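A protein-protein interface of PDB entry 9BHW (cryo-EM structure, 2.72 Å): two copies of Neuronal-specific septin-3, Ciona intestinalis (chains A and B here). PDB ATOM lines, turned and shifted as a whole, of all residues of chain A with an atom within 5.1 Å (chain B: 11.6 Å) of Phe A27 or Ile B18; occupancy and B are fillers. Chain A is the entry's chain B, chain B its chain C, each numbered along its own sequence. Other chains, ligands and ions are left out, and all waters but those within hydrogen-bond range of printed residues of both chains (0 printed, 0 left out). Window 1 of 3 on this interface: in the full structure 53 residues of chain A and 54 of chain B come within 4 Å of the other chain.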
ATOM      1  N   ALA A  22       4.435  26.944  13.778  1.00  0.00           N
ATOM      2  CA  ALA A  22       3.778  26.352  12.623  1.00  0.00           C
ATOM      3  C   ALA A  22       2.273  26.288  12.827  1.00  0.00           C
ATOM      4  O   ALA A  22       1.501  26.522  11.889  1.00  0.00           O
ATOM      5  CB  ALA A  22       4.344  24.962  12.355  1.00  0.00           C
ATOM      6  N   GLN A  25       0.313  29.167  11.330  1.00  0.00           N
ATOM      7  CA  GLN A  25       0.439  29.523   9.922  1.00  0.00           C
ATOM      8  C   GLN A  25      -0.085  28.441   8.996  1.00  0.00           C
ATOM      9  O   GLN A  25      -0.957  28.711   8.163  1.00  0.00           O
ATOM     10  CB  GLN A  25       1.906  29.826   9.585  1.00  0.00           C
ATOM     11  CG  GLN A  25       2.542  30.879  10.465  1.00  0.00           C
ATOM     12  CD  GLN A  25       4.054  30.788  10.480  1.00  0.00           C
ATOM     13  OE1 GLN A  25       4.643  29.940   9.808  1.00  0.00           O
ATOM     14  NE2 GLN A  25       4.693  31.662  11.250  1.00  0.00           N
ATOM     15  N   GLY A  26       0.415  27.227   9.120  1.00  0.00           N
ATOM     16  CA  GLY A  26       0.033  26.172   8.204  1.00  0.00           C
ATOM     17  C   GLY A  26       0.994  26.055   7.040  1.00  0.00           C
ATOM     18  O   GLY A  26       1.533  27.037   6.532  1.00  0.00           O
ATOM     19  N   PHE A  27       1.207  24.822   6.607  1.00  0.00           N
ATOM     20  CA  PHE A  27       2.138  24.522   5.536  1.00  0.00           C
ATOM     21  C   PHE A  27       1.426  24.523   4.192  1.00  0.00           C
ATOM     22  O   PHE A  27       0.289  24.068   4.064  1.00  0.00           O
ATOM     23  CB  PHE A  27       2.810  23.173   5.776  1.00  0.00           C
ATOM     24  CG  PHE A  27       3.492  23.072   7.105  1.00  0.00           C
ATOM     25  CD1 PHE A  27       4.808  23.468   7.254  1.00  0.00           C
ATOM     26  CD2 PHE A  27       2.820  22.581   8.208  1.00  0.00           C
ATOM     27  CE1 PHE A  27       5.436  23.375   8.476  1.00  0.00           C
ATOM     28  CE2 PHE A  27       3.445  22.486   9.429  1.00  0.00           C
ATOM     29  CZ  PHE A  27       4.753  22.882   9.563  1.00  0.00           C
ATOM     30  N   GLU A  28       2.120  25.032   3.181  1.00  0.00           N
ATOM     31  CA  GLU A  28       1.572  25.181   1.842  1.00  0.00           C
ATOM     32  C   GLU A  28       2.139  24.088   0.954  1.00  0.00           C
ATOM     33  O   GLU A  28       3.358  23.900   0.901  1.00  0.00           O
ATOM     34  CB  GLU A  28       1.906  26.556   1.268  1.00  0.00           C
ATOM     35  CG  GLU A  28       0.971  27.651   1.713  1.00  0.00           C
ATOM     36  CD  GLU A  28       1.504  29.029   1.402  1.00  0.00           C
ATOM     37  OE1 GLU A  28       0.797  29.805   0.729  1.00  0.00           O
ATOM     38  OE2 GLU A  28       2.633  29.339   1.834  1.00  0.00           O
ATOM     39  N   PHE A  29       1.261  23.368   0.262  1.00  0.00           N
ATOM     40  CA  PHE A  29       1.682  22.289  -0.620  1.00  0.00           C
ATOM     41  C   PHE A  29       0.942  22.407  -1.942  1.00  0.00           C
ATOM     42  O   PHE A  29      -0.286  22.550  -1.967  1.00  0.00           O
ATOM     43  CB  PHE A  29       1.444  20.930   0.036  1.00  0.00           C
ATOM     44  CG  PHE A  29       2.159  19.799  -0.629  1.00  0.00           C
ATOM     45  CD1 PHE A  29       3.531  19.811  -0.746  1.00  0.00           C
ATOM     46  CD2 PHE A  29       1.470  18.691  -1.074  1.00  0.00           C
ATOM     47  CE1 PHE A  29       4.198  18.767  -1.343  1.00  0.00           C
ATOM     48  CE2 PHE A  29       2.136  17.641  -1.660  1.00  0.00           C
ATOM     49  CZ  PHE A  29       3.499  17.683  -1.798  1.00  0.00           C
ATOM     50  N   ILE A  82      -2.267  20.192  12.335  1.00  0.00           N
ATOM     51  CA  ILE A  82      -1.456  20.622  11.206  1.00  0.00           C
ATOM     52  C   ILE A  82      -2.389  20.983  10.062  1.00  0.00           C
ATOM     53  O   ILE A  82      -3.202  20.158   9.628  1.00  0.00           O
ATOM     54  CB  ILE A  82      -0.451  19.541  10.787  1.00  0.00           C
ATOM     55  CG1 ILE A  82       0.549  19.296  11.913  1.00  0.00           C
ATOM     56  CG2 ILE A  82       0.286  19.965   9.535  1.00  0.00           C
ATOM     57  CD1 ILE A  82       1.674  18.378  11.538  1.00  0.00           C
ATOM     58  N   LEU A  83      -2.281  22.221   9.590  1.00  0.00           N
ATOM     59  CA  LEU A  83      -3.065  22.721   8.472  1.00  0.00           C
ATOM     60  C   LEU A  83      -2.220  22.686   7.208  1.00  0.00           C
ATOM     61  O   LEU A  83      -1.060  23.110   7.217  1.00  0.00           O
ATOM     62  CB  LEU A  83      -3.545  24.148   8.729  1.00  0.00           C
ATOM     63  CG  LEU A  83      -4.939  24.349   9.309  1.00  0.00           C
ATOM     64  CD1 LEU A  83      -5.002  23.859  10.746  1.00  0.00           C
ATOM     65  CD2 LEU A  83      -5.327  25.810   9.217  1.00  0.00           C
ATOM     66  N   LEU A  84      -2.805  22.188   6.125  1.00  0.00           N
ATOM     67  CA  LEU A  84      -2.158  22.138   4.824  1.00  0.00           C
ATOM     68  C   LEU A  84      -3.024  22.921   3.852  1.00  0.00           C
ATOM     69  O   LEU A  84      -4.166  22.535   3.578  1.00  0.00           O
ATOM     70  CB  LEU A  84      -1.963  20.700   4.356  1.00  0.00           C
ATOM     71  CG  LEU A  84      -0.983  20.485   3.206  1.00  0.00           C
ATOM     72  CD1 LEU A  84       0.438  20.722   3.672  1.00  0.00           C
ATOM     73  CD2 LEU A  84      -1.127  19.091   2.643  1.00  0.00           C
ATOM     74  N   LYS A  85      -2.491  24.034   3.368  1.00  0.00           N
ATOM     75  CA  LYS A  85      -3.091  24.789   2.278  1.00  0.00           C
ATOM     76  C   LYS A  85      -2.638  24.136   0.981  1.00  0.00           C
ATOM     77  O   LYS A  85      -1.483  24.285   0.568  1.00  0.00           O
ATOM     78  CB  LYS A  85      -2.671  26.253   2.350  1.00  0.00           C
ATOM     79  CG  LYS A  85      -3.197  26.975   3.569  1.00  0.00           C
ATOM     80  CD  LYS A  85      -2.765  28.424   3.586  1.00  0.00           C
ATOM     81  CE  LYS A  85      -3.373  29.162   4.764  1.00  0.00           C
ATOM     82  NZ  LYS A  85      -2.840  28.661   6.061  1.00  0.00           N
ATOM     83  N   GLN A 276       8.690  17.381   2.865  1.00  0.00           N
ATOM     84  CA  GLN A 276       9.573  18.505   3.133  1.00  0.00           C
ATOM     85  C   GLN A 276      10.788  18.486   2.220  1.00  0.00           C
ATOM     86  O   GLN A 276      11.314  19.547   1.875  1.00  0.00           O
ATOM     87  CB  GLN A 276       9.996  18.497   4.598  1.00  0.00           C
ATOM     88  CG  GLN A 276      10.678  19.767   5.058  1.00  0.00           C
ATOM     89  CD  GLN A 276       9.835  21.001   4.844  1.00  0.00           C
ATOM     90  OE1 GLN A 276       8.612  20.959   4.950  1.00  0.00           O
ATOM     91  NE2 GLN A 276      10.487  22.115   4.547  1.00  0.00           N
ATOM     92  N   LYS A 279       9.588  20.138  -0.914  1.00  0.00           N
ATOM     93  CA  LYS A 279       9.537  21.587  -0.740  1.00  0.00           C
ATOM     94  C   LYS A 279      10.933  22.200  -0.749  1.00  0.00           C
ATOM     95  O   LYS A 279      11.154  23.254  -1.358  1.00  0.00           O
ATOM     96  CB  LYS A 279       8.804  21.934   0.553  1.00  0.00           C
ATOM     97  CG  LYS A 279       7.319  21.648   0.518  1.00  0.00           C
ATOM     98  CD  LYS A 279       6.613  22.248   1.714  1.00  0.00           C
ATOM     99  CE  LYS A 279       6.562  23.756   1.614  1.00  0.00           C
ATOM    100  NZ  LYS A 279       5.655  24.342   2.631  1.00  0.00           N
ATOM    101  N   GLY B  10      -1.660  11.293   6.582  1.00  0.00           N
ATOM    102  CA  GLY B  10      -0.298  11.337   7.065  1.00  0.00           C
ATOM    103  C   GLY B  10       0.347  12.704   7.130  1.00  0.00           C
ATOM    104  O   GLY B  10       1.572  12.777   7.262  1.00  0.00           O
ATOM    105  N   ILE B  11      -0.430  13.784   7.040  1.00  0.00           N
ATOM    106  CA  ILE B  11       0.144  15.126   7.087  1.00  0.00           C
ATOM    107  C   ILE B  11       0.827  15.376   8.424  1.00  0.00           C
ATOM    108  O   ILE B  11       1.826  16.105   8.495  1.00  0.00           O
ATOM    109  CB  ILE B  11      -0.942  16.179   6.800  1.00  0.00           C
ATOM    110  CG1 ILE B  11      -1.492  15.998   5.393  1.00  0.00           C
ATOM    111  CG2 ILE B  11      -0.392  17.576   6.934  1.00  0.00           C
ATOM    112  CD1 ILE B  11      -2.665  16.884   5.095  1.00  0.00           C
ATOM    113  N   ASP B  12       0.325  14.758   9.494  1.00  0.00           N
ATOM    114  CA  ASP B  12       0.878  14.978  10.825  1.00  0.00           C
ATOM    115  C   ASP B  12       2.350  14.601  10.919  1.00  0.00           C
ATOM    116  O   ASP B  12       3.043  15.083  11.821  1.00  0.00           O
ATOM    117  CB  ASP B  12       0.067  14.196  11.859  1.00  0.00           C
ATOM    118  CG  ASP B  12       0.120  12.693  11.641  1.00  0.00           C
ATOM    119  OD1 ASP B  12       0.750  12.239  10.663  1.00  0.00           O
ATOM    120  OD2 ASP B  12      -0.468  11.957  12.457  1.00  0.00           O
ATOM    121  N   THR B  13       2.843  13.754  10.015  1.00  0.00           N
ATOM    122  CA  THR B  13       4.246  13.362  10.040  1.00  0.00           C
ATOM    123  C   THR B  13       5.167  14.530   9.713  1.00  0.00           C
ATOM    124  O   THR B  13       6.352  14.491  10.066  1.00  0.00           O
ATOM    125  CB  THR B  13       4.465  12.203   9.064  1.00  0.00           C
ATOM    126  OG1 THR B  13       3.626  11.106   9.443  1.00  0.00           O
ATOM    127  CG2 THR B  13       5.903  11.718   9.090  1.00  0.00           C
ATOM    128  N   LEU B  14       4.625  15.593   9.113  1.00  0.00           N
ATOM    129  CA  LEU B  14       5.442  16.688   8.599  1.00  0.00           C
ATOM    130  C   LEU B  14       6.417  17.209   9.643  1.00  0.00           C
ATOM    131  O   LEU B  14       7.612  17.373   9.363  1.00  0.00           O
ATOM    132  CB  LEU B  14       4.534  17.812   8.111  1.00  0.00           C
ATOM    133  CG  LEU B  14       5.133  18.754   7.076  1.00  0.00           C
ATOM    134  CD1 LEU B  14       5.777  17.957   5.965  1.00  0.00           C
ATOM    135  CD2 LEU B  14       4.053  19.663   6.534  1.00  0.00           C
ATOM    136  N   THR B  15       5.930  17.450  10.861  1.00  0.00           N
ATOM    137  CA  THR B  15       6.787  17.980  11.916  1.00  0.00           C
ATOM    138  C   THR B  15       8.022  17.112  12.104  1.00  0.00           C
ATOM    139  O   THR B  15       9.156  17.610  12.077  1.00  0.00           O
ATOM    140  CB  THR B  15       6.002  18.090  13.221  1.00  0.00           C
ATOM    141  OG1 THR B  15       4.886  18.966  13.031  1.00  0.00           O
ATOM    142  CG2 THR B  15       6.885  18.642  14.325  1.00  0.00           C
ATOM    143  N   GLU B  16       7.822  15.799  12.243  1.00  0.00           N
ATOM    144  CA  GLU B  16       8.955  14.890  12.373  1.00  0.00           C
ATOM    145  C   GLU B  16       9.931  15.065  11.220  1.00  0.00           C
ATOM    146  O   GLU B  16      11.143  15.180  11.438  1.00  0.00           O
ATOM    147  CB  GLU B  16       8.463  13.448  12.447  1.00  0.00           C
ATOM    148  CG  GLU B  16       9.560  12.415  12.350  1.00  0.00           C
ATOM    149  CD  GLU B  16      10.237  12.152  13.675  1.00  0.00           C
ATOM    150  OE1 GLU B  16       9.965  12.889  14.645  1.00  0.00           O
ATOM    151  OE2 GLU B  16      11.046  11.204  13.749  1.00  0.00           O
ATOM    152  N   GLN B  17       9.414  15.133   9.991  1.00  0.00           N
ATOM    153  CA  GLN B  17      10.274  15.361   8.835  1.00  0.00           C
ATOM    154  C   GLN B  17      11.130  16.599   9.041  1.00  0.00           C
ATOM    155  O   GLN B  17      12.360  16.546   8.913  1.00  0.00           O
ATOM    156  CB  GLN B  17       9.429  15.499   7.571  1.00  0.00           C
ATOM    157  CG  GLN B  17       8.635  14.262   7.216  1.00  0.00           C
ATOM    158  CD  GLN B  17       7.744  14.478   6.019  1.00  0.00           C
ATOM    159  OE1 GLN B  17       8.097  15.205   5.095  1.00  0.00           O
ATOM    160  NE2 GLN B  17       6.577  13.851   6.028  1.00  0.00           N
ATOM    161  N   ILE B  18      10.498  17.706   9.435  1.00  0.00           N
ATOM    162  CA  ILE B  18      11.238  18.943   9.649  1.00  0.00           C
ATOM    163  C   ILE B  18      12.339  18.724  10.671  1.00  0.00           C
ATOM    164  O   ILE B  18      13.476  19.178  10.488  1.00  0.00           O
ATOM    165  CB  ILE B  18      10.287  20.075  10.072  1.00  0.00           C
ATOM    166  CG1 ILE B  18       9.309  20.391   8.946  1.00  0.00           C
ATOM    167  CG2 ILE B  18      11.071  21.316  10.453  1.00  0.00           C
ATOM    168  CD1 ILE B  18       8.255  21.378   9.330  1.00  0.00           C
ATOM    169  N   ARG B  19      12.036  17.984  11.741  1.00  0.00           N
ATOM    170  CA  ARG B  19      13.049  17.719  12.750  1.00  0.00           C
ATOM    171  C   ARG B  19      14.259  17.042  12.126  1.00  0.00           C
ATOM    172  O   ARG B  19      15.399  17.484  12.315  1.00  0.00           O
ATOM    173  CB  ARG B  19      12.471  16.855  13.869  1.00  0.00           C
ATOM    174  CG  ARG B  19      13.449  16.615  14.999  1.00  0.00           C
ATOM    175  CD  ARG B  19      12.863  15.738  16.077  1.00  0.00           C
ATOM    176  NE  ARG B  19      12.570  14.401  15.579  1.00  0.00           N
ATOM    177  CZ  ARG B  19      13.468  13.433  15.474  1.00  0.00           C
ATOM    178  NH1 ARG B  19      14.732  13.625  15.803  1.00  0.00           N
ATOM    179  NH2 ARG B  19      13.087  12.241  15.025  1.00  0.00           N
ATOM    180  N   LYS B  20      14.025  16.002  11.321  1.00  0.00           N
ATOM    181  CA  LYS B  20      15.143  15.282  10.728  1.00  0.00           C
ATOM    182  C   LYS B  20      15.958  16.165   9.801  1.00  0.00           C
ATOM    183  O   LYS B  20      17.124  15.858   9.537  1.00  0.00           O
ATOM    184  CB  LYS B  20      14.658  14.055   9.963  1.00  0.00           C
ATOM    185  CG  LYS B  20      14.058  12.969  10.819  1.00  0.00           C
ATOM    186  CD  LYS B  20      13.592  11.817   9.945  1.00  0.00           C
ATOM    187  CE  LYS B  20      13.002  10.683  10.759  1.00  0.00           C
ATOM    188  NZ  LYS B  20      12.529   9.574   9.896  1.00  0.00           N
ATOM    189  N   LYS B  21      15.380  17.253   9.309  1.00  0.00           N
ATOM    190  CA  LYS B  21      16.118  18.153   8.444  1.00  0.00           C
ATOM    191  C   LYS B  21      16.841  19.243   9.214  1.00  0.00           C
ATOM    192  O   LYS B  21      17.788  19.834   8.683  1.00  0.00           O
ATOM    193  CB  LYS B  21      15.180  18.775   7.412  1.00  0.00           C
ATOM    194  CG  LYS B  21      14.795  17.805   6.322  1.00  0.00           C
ATOM    195  CD  LYS B  21      14.147  18.504   5.162  1.00  0.00           C
ATOM    196  CE  LYS B  21      14.200  17.626   3.938  1.00  0.00           C
ATOM    197  NZ  LYS B  21      15.555  17.045   3.766  1.00  0.00           N
ATOM    198  N   ALA B  22      16.418  19.531  10.444  1.00  0.00           N
ATOM    199  CA  ALA B  22      17.190  20.435  11.282  1.00  0.00           C
ATOM    200  C   ALA B  22      18.328  19.697  11.971  1.00  0.00           C
ATOM    201  O   ALA B  22      19.405  20.266  12.188  1.00  0.00           O
ATOM    202  CB  ALA B  22      16.282  21.104  12.307  1.00  0.00           C
ATOM    203  N   LEU B  23      18.111  18.416  12.274  1.00  0.00           N
ATOM    204  CA  LEU B  23      19.064  17.626  13.044  1.00  0.00           C
ATOM    205  C   LEU B  23      20.446  17.621  12.413  1.00  0.00           C
ATOM    206  O   LEU B  23      21.454  17.587  13.127  1.00  0.00           O
ATOM    207  CB  LEU B  23      18.542  16.196  13.180  1.00  0.00           C
ATOM    208  CG  LEU B  23      19.332  15.177  13.995  1.00  0.00           C
ATOM    209  CD1 LEU B  23      19.292  15.518  15.472  1.00  0.00           C
ATOM    210  CD2 LEU B  23      18.794  13.781  13.744  1.00  0.00           C
ATOM    211  N   ARG B  24      20.519  17.653  11.089  1.00  0.00           N
ATOM    212  CA  ARG B  24      21.798  17.625  10.402  1.00  0.00           C
ATOM    213  C   ARG B  24      22.455  18.994  10.295  1.00  0.00           C
ATOM    214  O   ARG B  24      23.684  19.067  10.202  1.00  0.00           O
ATOM    215  CB  ARG B  24      21.627  17.033   9.001  1.00  0.00           C
ATOM    216  CG  ARG B  24      20.608  17.758   8.140  1.00  0.00           C
ATOM    217  CD  ARG B  24      20.723  17.349   6.682  1.00  0.00           C
ATOM    218  NE  ARG B  24      19.779  18.071   5.837  1.00  0.00           N
ATOM    219  CZ  ARG B  24      19.463  17.722   4.598  1.00  0.00           C
ATOM    220  NH1 ARG B  24      19.998  16.658   4.021  1.00  0.00           N
ATOM    221  NH2 ARG B  24      18.585  18.457   3.921  1.00  0.00           N
ATOM    222  N   GLN B  25      21.679  20.074  10.317  1.00  0.00           N
ATOM    223  CA  GLN B  25      22.226  21.405  10.084  1.00  0.00           C
ATOM    224  C   GLN B  25      22.418  22.204  11.361  1.00  0.00           C
ATOM    225  O   GLN B  25      23.320  23.042  11.431  1.00  0.00           O
ATOM    226  CB  GLN B  25      21.321  22.188   9.131  1.00  0.00           C
ATOM    227  CG  GLN B  25      21.179  21.562   7.761  1.00  0.00           C
ATOM    228  CD  GLN B  25      20.174  22.288   6.894  1.00  0.00           C
ATOM    229  OE1 GLN B  25      20.213  22.196   5.668  1.00  0.00           O
ATOM    230  NE2 GLN B  25      19.265  23.020   7.529  1.00  0.00           N
ATOM    231  N   GLY B  26      21.589  21.972  12.366  1.00  0.00           N
ATOM    232  CA  GLY B  26      21.690  22.690  13.614  1.00  0.00           C
ATOM    233  C   GLY B  26      21.114  24.090  13.519  1.00  0.00           C
ATOM    234  O   GLY B  26      20.962  24.667  12.446  1.00  0.00           O
ATOM    235  N   PHE B  27      20.788  24.639  14.679  1.00  0.00           N
ATOM    236  CA  PHE B  27      20.266  25.991  14.777  1.00  0.00           C
ATOM    237  C   PHE B  27      21.384  26.931  15.189  1.00  0.00           C
ATOM    238  O   PHE B  27      22.440  26.501  15.644  1.00  0.00           O
ATOM    239  CB  PHE B  27      19.116  26.058  15.779  1.00  0.00           C
ATOM    240  CG  PHE B  27      18.076  25.003  15.567  1.00  0.00           C
ATOM    241  CD1 PHE B  27      16.998  25.236  14.737  1.00  0.00           C
ATOM    242  CD2 PHE B  27      18.182  23.773  16.188  1.00  0.00           C
ATOM    243  CE1 PHE B  27      16.046  24.268  14.538  1.00  0.00           C
ATOM    244  CE2 PHE B  27      17.232  22.802  15.989  1.00  0.00           C
ATOM    245  CZ  PHE B  27      16.161  23.051  15.167  1.00  0.00           C
ATOM    246  N   GLY B  81      21.199  15.756  20.929  1.00  0.00           N
ATOM    247  CA  GLY B  81      21.173  15.685  19.489  1.00  0.00           C
ATOM    248  C   GLY B  81      21.053  17.013  18.782  1.00  0.00           C
ATOM    249  O   GLY B  81      21.289  17.071  17.569  1.00  0.00           O
ATOM    250  N   ILE B  82      20.713  18.084  19.491  1.00  0.00           N
ATOM    251  CA  ILE B  82      20.522  19.394  18.882  1.00  0.00           C
ATOM    252  C   ILE B  82      21.810  20.195  18.983  1.00  0.00           C
ATOM    253  O   ILE B  82      22.387  20.334  20.071  1.00  0.00           O
ATOM    254  CB  ILE B  82      19.338  20.137  19.521  1.00  0.00           C
ATOM    255  CG1 ILE B  82      18.052  19.358  19.255  1.00  0.00           C
ATOM    256  CG2 ILE B  82      19.230  21.549  18.985  1.00  0.00           C
ATOM    257  CD1 ILE B  82      16.869  19.837  20.028  1.00  0.00           C
ATOM    258  N   LEU B  83      22.268  20.703  17.841  1.00  0.00           N
ATOM    259  CA  LEU B  83      23.449  21.548  17.742  1.00  0.00           C
ATOM    260  C   LEU B  83      23.030  23.008  17.738  1.00  0.00           C
ATOM    261  O   LEU B  83      22.161  23.408  16.955  1.00  0.00           O
ATOM    262  CB  LEU B  83      24.242  21.245  16.471  1.00  0.00           C
ATOM    263  CG  LEU B  83      24.931  19.905  16.276  1.00  0.00           C
ATOM    264  CD1 LEU B  83      25.512  19.823  14.879  1.00  0.00           C
ATOM    265  CD2 LEU B  83      26.040  19.803  17.284  1.00  0.00           C
ATOM    266  N   ARG B 130      21.591  28.441   1.769  1.00  0.00           N
ATOM    267  CA  ARG B 130      21.302  28.838   3.141  1.00  0.00           C
ATOM    268  C   ARG B 130      22.294  29.917   3.544  1.00  0.00           C
ATOM    269  O   ARG B 130      23.491  29.643   3.684  1.00  0.00           O
ATOM    270  CB  ARG B 130      21.380  27.639   4.083  1.00  0.00           C
ATOM    271  CG  ARG B 130      20.139  26.764   4.083  1.00  0.00           C
ATOM    272  CD  ARG B 130      20.317  25.560   4.994  1.00  0.00           C
ATOM    273  NE  ARG B 130      19.596  24.383   4.519  1.00  0.00           N
ATOM    274  CZ  ARG B 130      18.275  24.263   4.495  1.00  0.00           C
ATOM    275  NH1 ARG B 130      17.483  25.225   4.940  1.00  0.00           N
ATOM    276  NH2 ARG B 130      17.734  23.144   4.022  1.00  0.00           N
ATOM    277  N   GLN B 276      13.015  31.280  19.372  1.00  0.00           N
ATOM    278  CA  GLN B 276      12.577  31.377  17.991  1.00  0.00           C
ATOM    279  C   GLN B 276      11.774  32.645  17.757  1.00  0.00           C
ATOM    280  O   GLN B 276      11.794  33.190  16.652  1.00  0.00           O
ATOM    281  CB  GLN B 276      11.772  30.141  17.609  1.00  0.00           C
ATOM    282  CG  GLN B 276      11.391  30.082  16.149  1.00  0.00           C
ATOM    283  CD  GLN B 276      12.598  30.041  15.246  1.00  0.00           C
ATOM    284  OE1 GLN B 276      13.270  29.018  15.139  1.00  0.00           O
ATOM    285  NE2 GLN B 276      12.879  31.153  14.582  1.00  0.00           N
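The backbone NH of Phe A27 is in hydrogen-bond range of the backbone carbonyl oxygen of Leu A83 (2.9 Å). The backbone carbonyl oxygen (O) of Phe A27 lies within hydrogen-bond range of the backbone NH (N) of Lys A85 (2.9 Å). OG1 of Thr B13 sits at hydrogen-bond distance from OD1 of Asp B12 (3.3 Å).
Ile B18 touches one residue of chain A. No residue of chain B comes within 4 Å of Ala A22. Gly A26 touches none of the printed residues of chain B. No residue of chain B comes within 4 Å of Glu A28. Of chain B, only Ile B11, Asp B12 and Thr B15 come within 4 Å of Ile A82. Leu A83 touches none of the printed residues of chain B. Of chain B, only Ile B11 comes within 4 Å of Leu A84. Lys A85 touches none of the printed residues of chain B. Gln A276 touches two residues of chain B. Of the printed residues of chain A, Gln B17 touches Gln A276 (3.2 Å). Printed residues of chain A within 4 Å of Lys B21: Gln A276 (3.7 Å). Of the printed residues of chain A, Ile B11 touches Ile A82 (3.6 Å) and Leu A84 (3.6 Å). Arg B130 touches none of the printed residues of chain A. Ile B82 touches none of the printed residues of chain A. The nearest printed residue of chain A that does not touch Gln B17 is Lys A279 (7.9 Å).
Phe A27 touches Leu B14 (CG to CD2, 3.5 Å). Phe A27 touches Ile B18 (CE1 to CD1, 3.6 Å). CG2 of Ile B11 touches CG2 of Ile A82, 3.6 Å away. Asp B12 touches Ile A82. Ile A82 touches Thr B15. Leu A84 touches Ile B11. Gln A276 touches Lys B21.
The side-chain amide oxygen (OE1) of Gln B17 lies within hydrogen-bond range of the backbone NH (N) of Gln A276 (3.2 Å).
7 positions are printed for both chains.
Of the 23 printed residues of chain B, 7 touch a printed residue of chain A. Of the 12 printed residues of chain A, 4 touch a printed residue of chain B. Hydrophobic or aromatic side chains of chain A within 4 Å of the printed part of chain B: Phe A27, Ile A82 and Leu A84. Among the printed residues, 8 pairs touch across the chains. Among the printed residues, no Asp or Glu carboxylate lies within 4 Å of a Lys or Arg side-chain nitrogen of the other chain.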
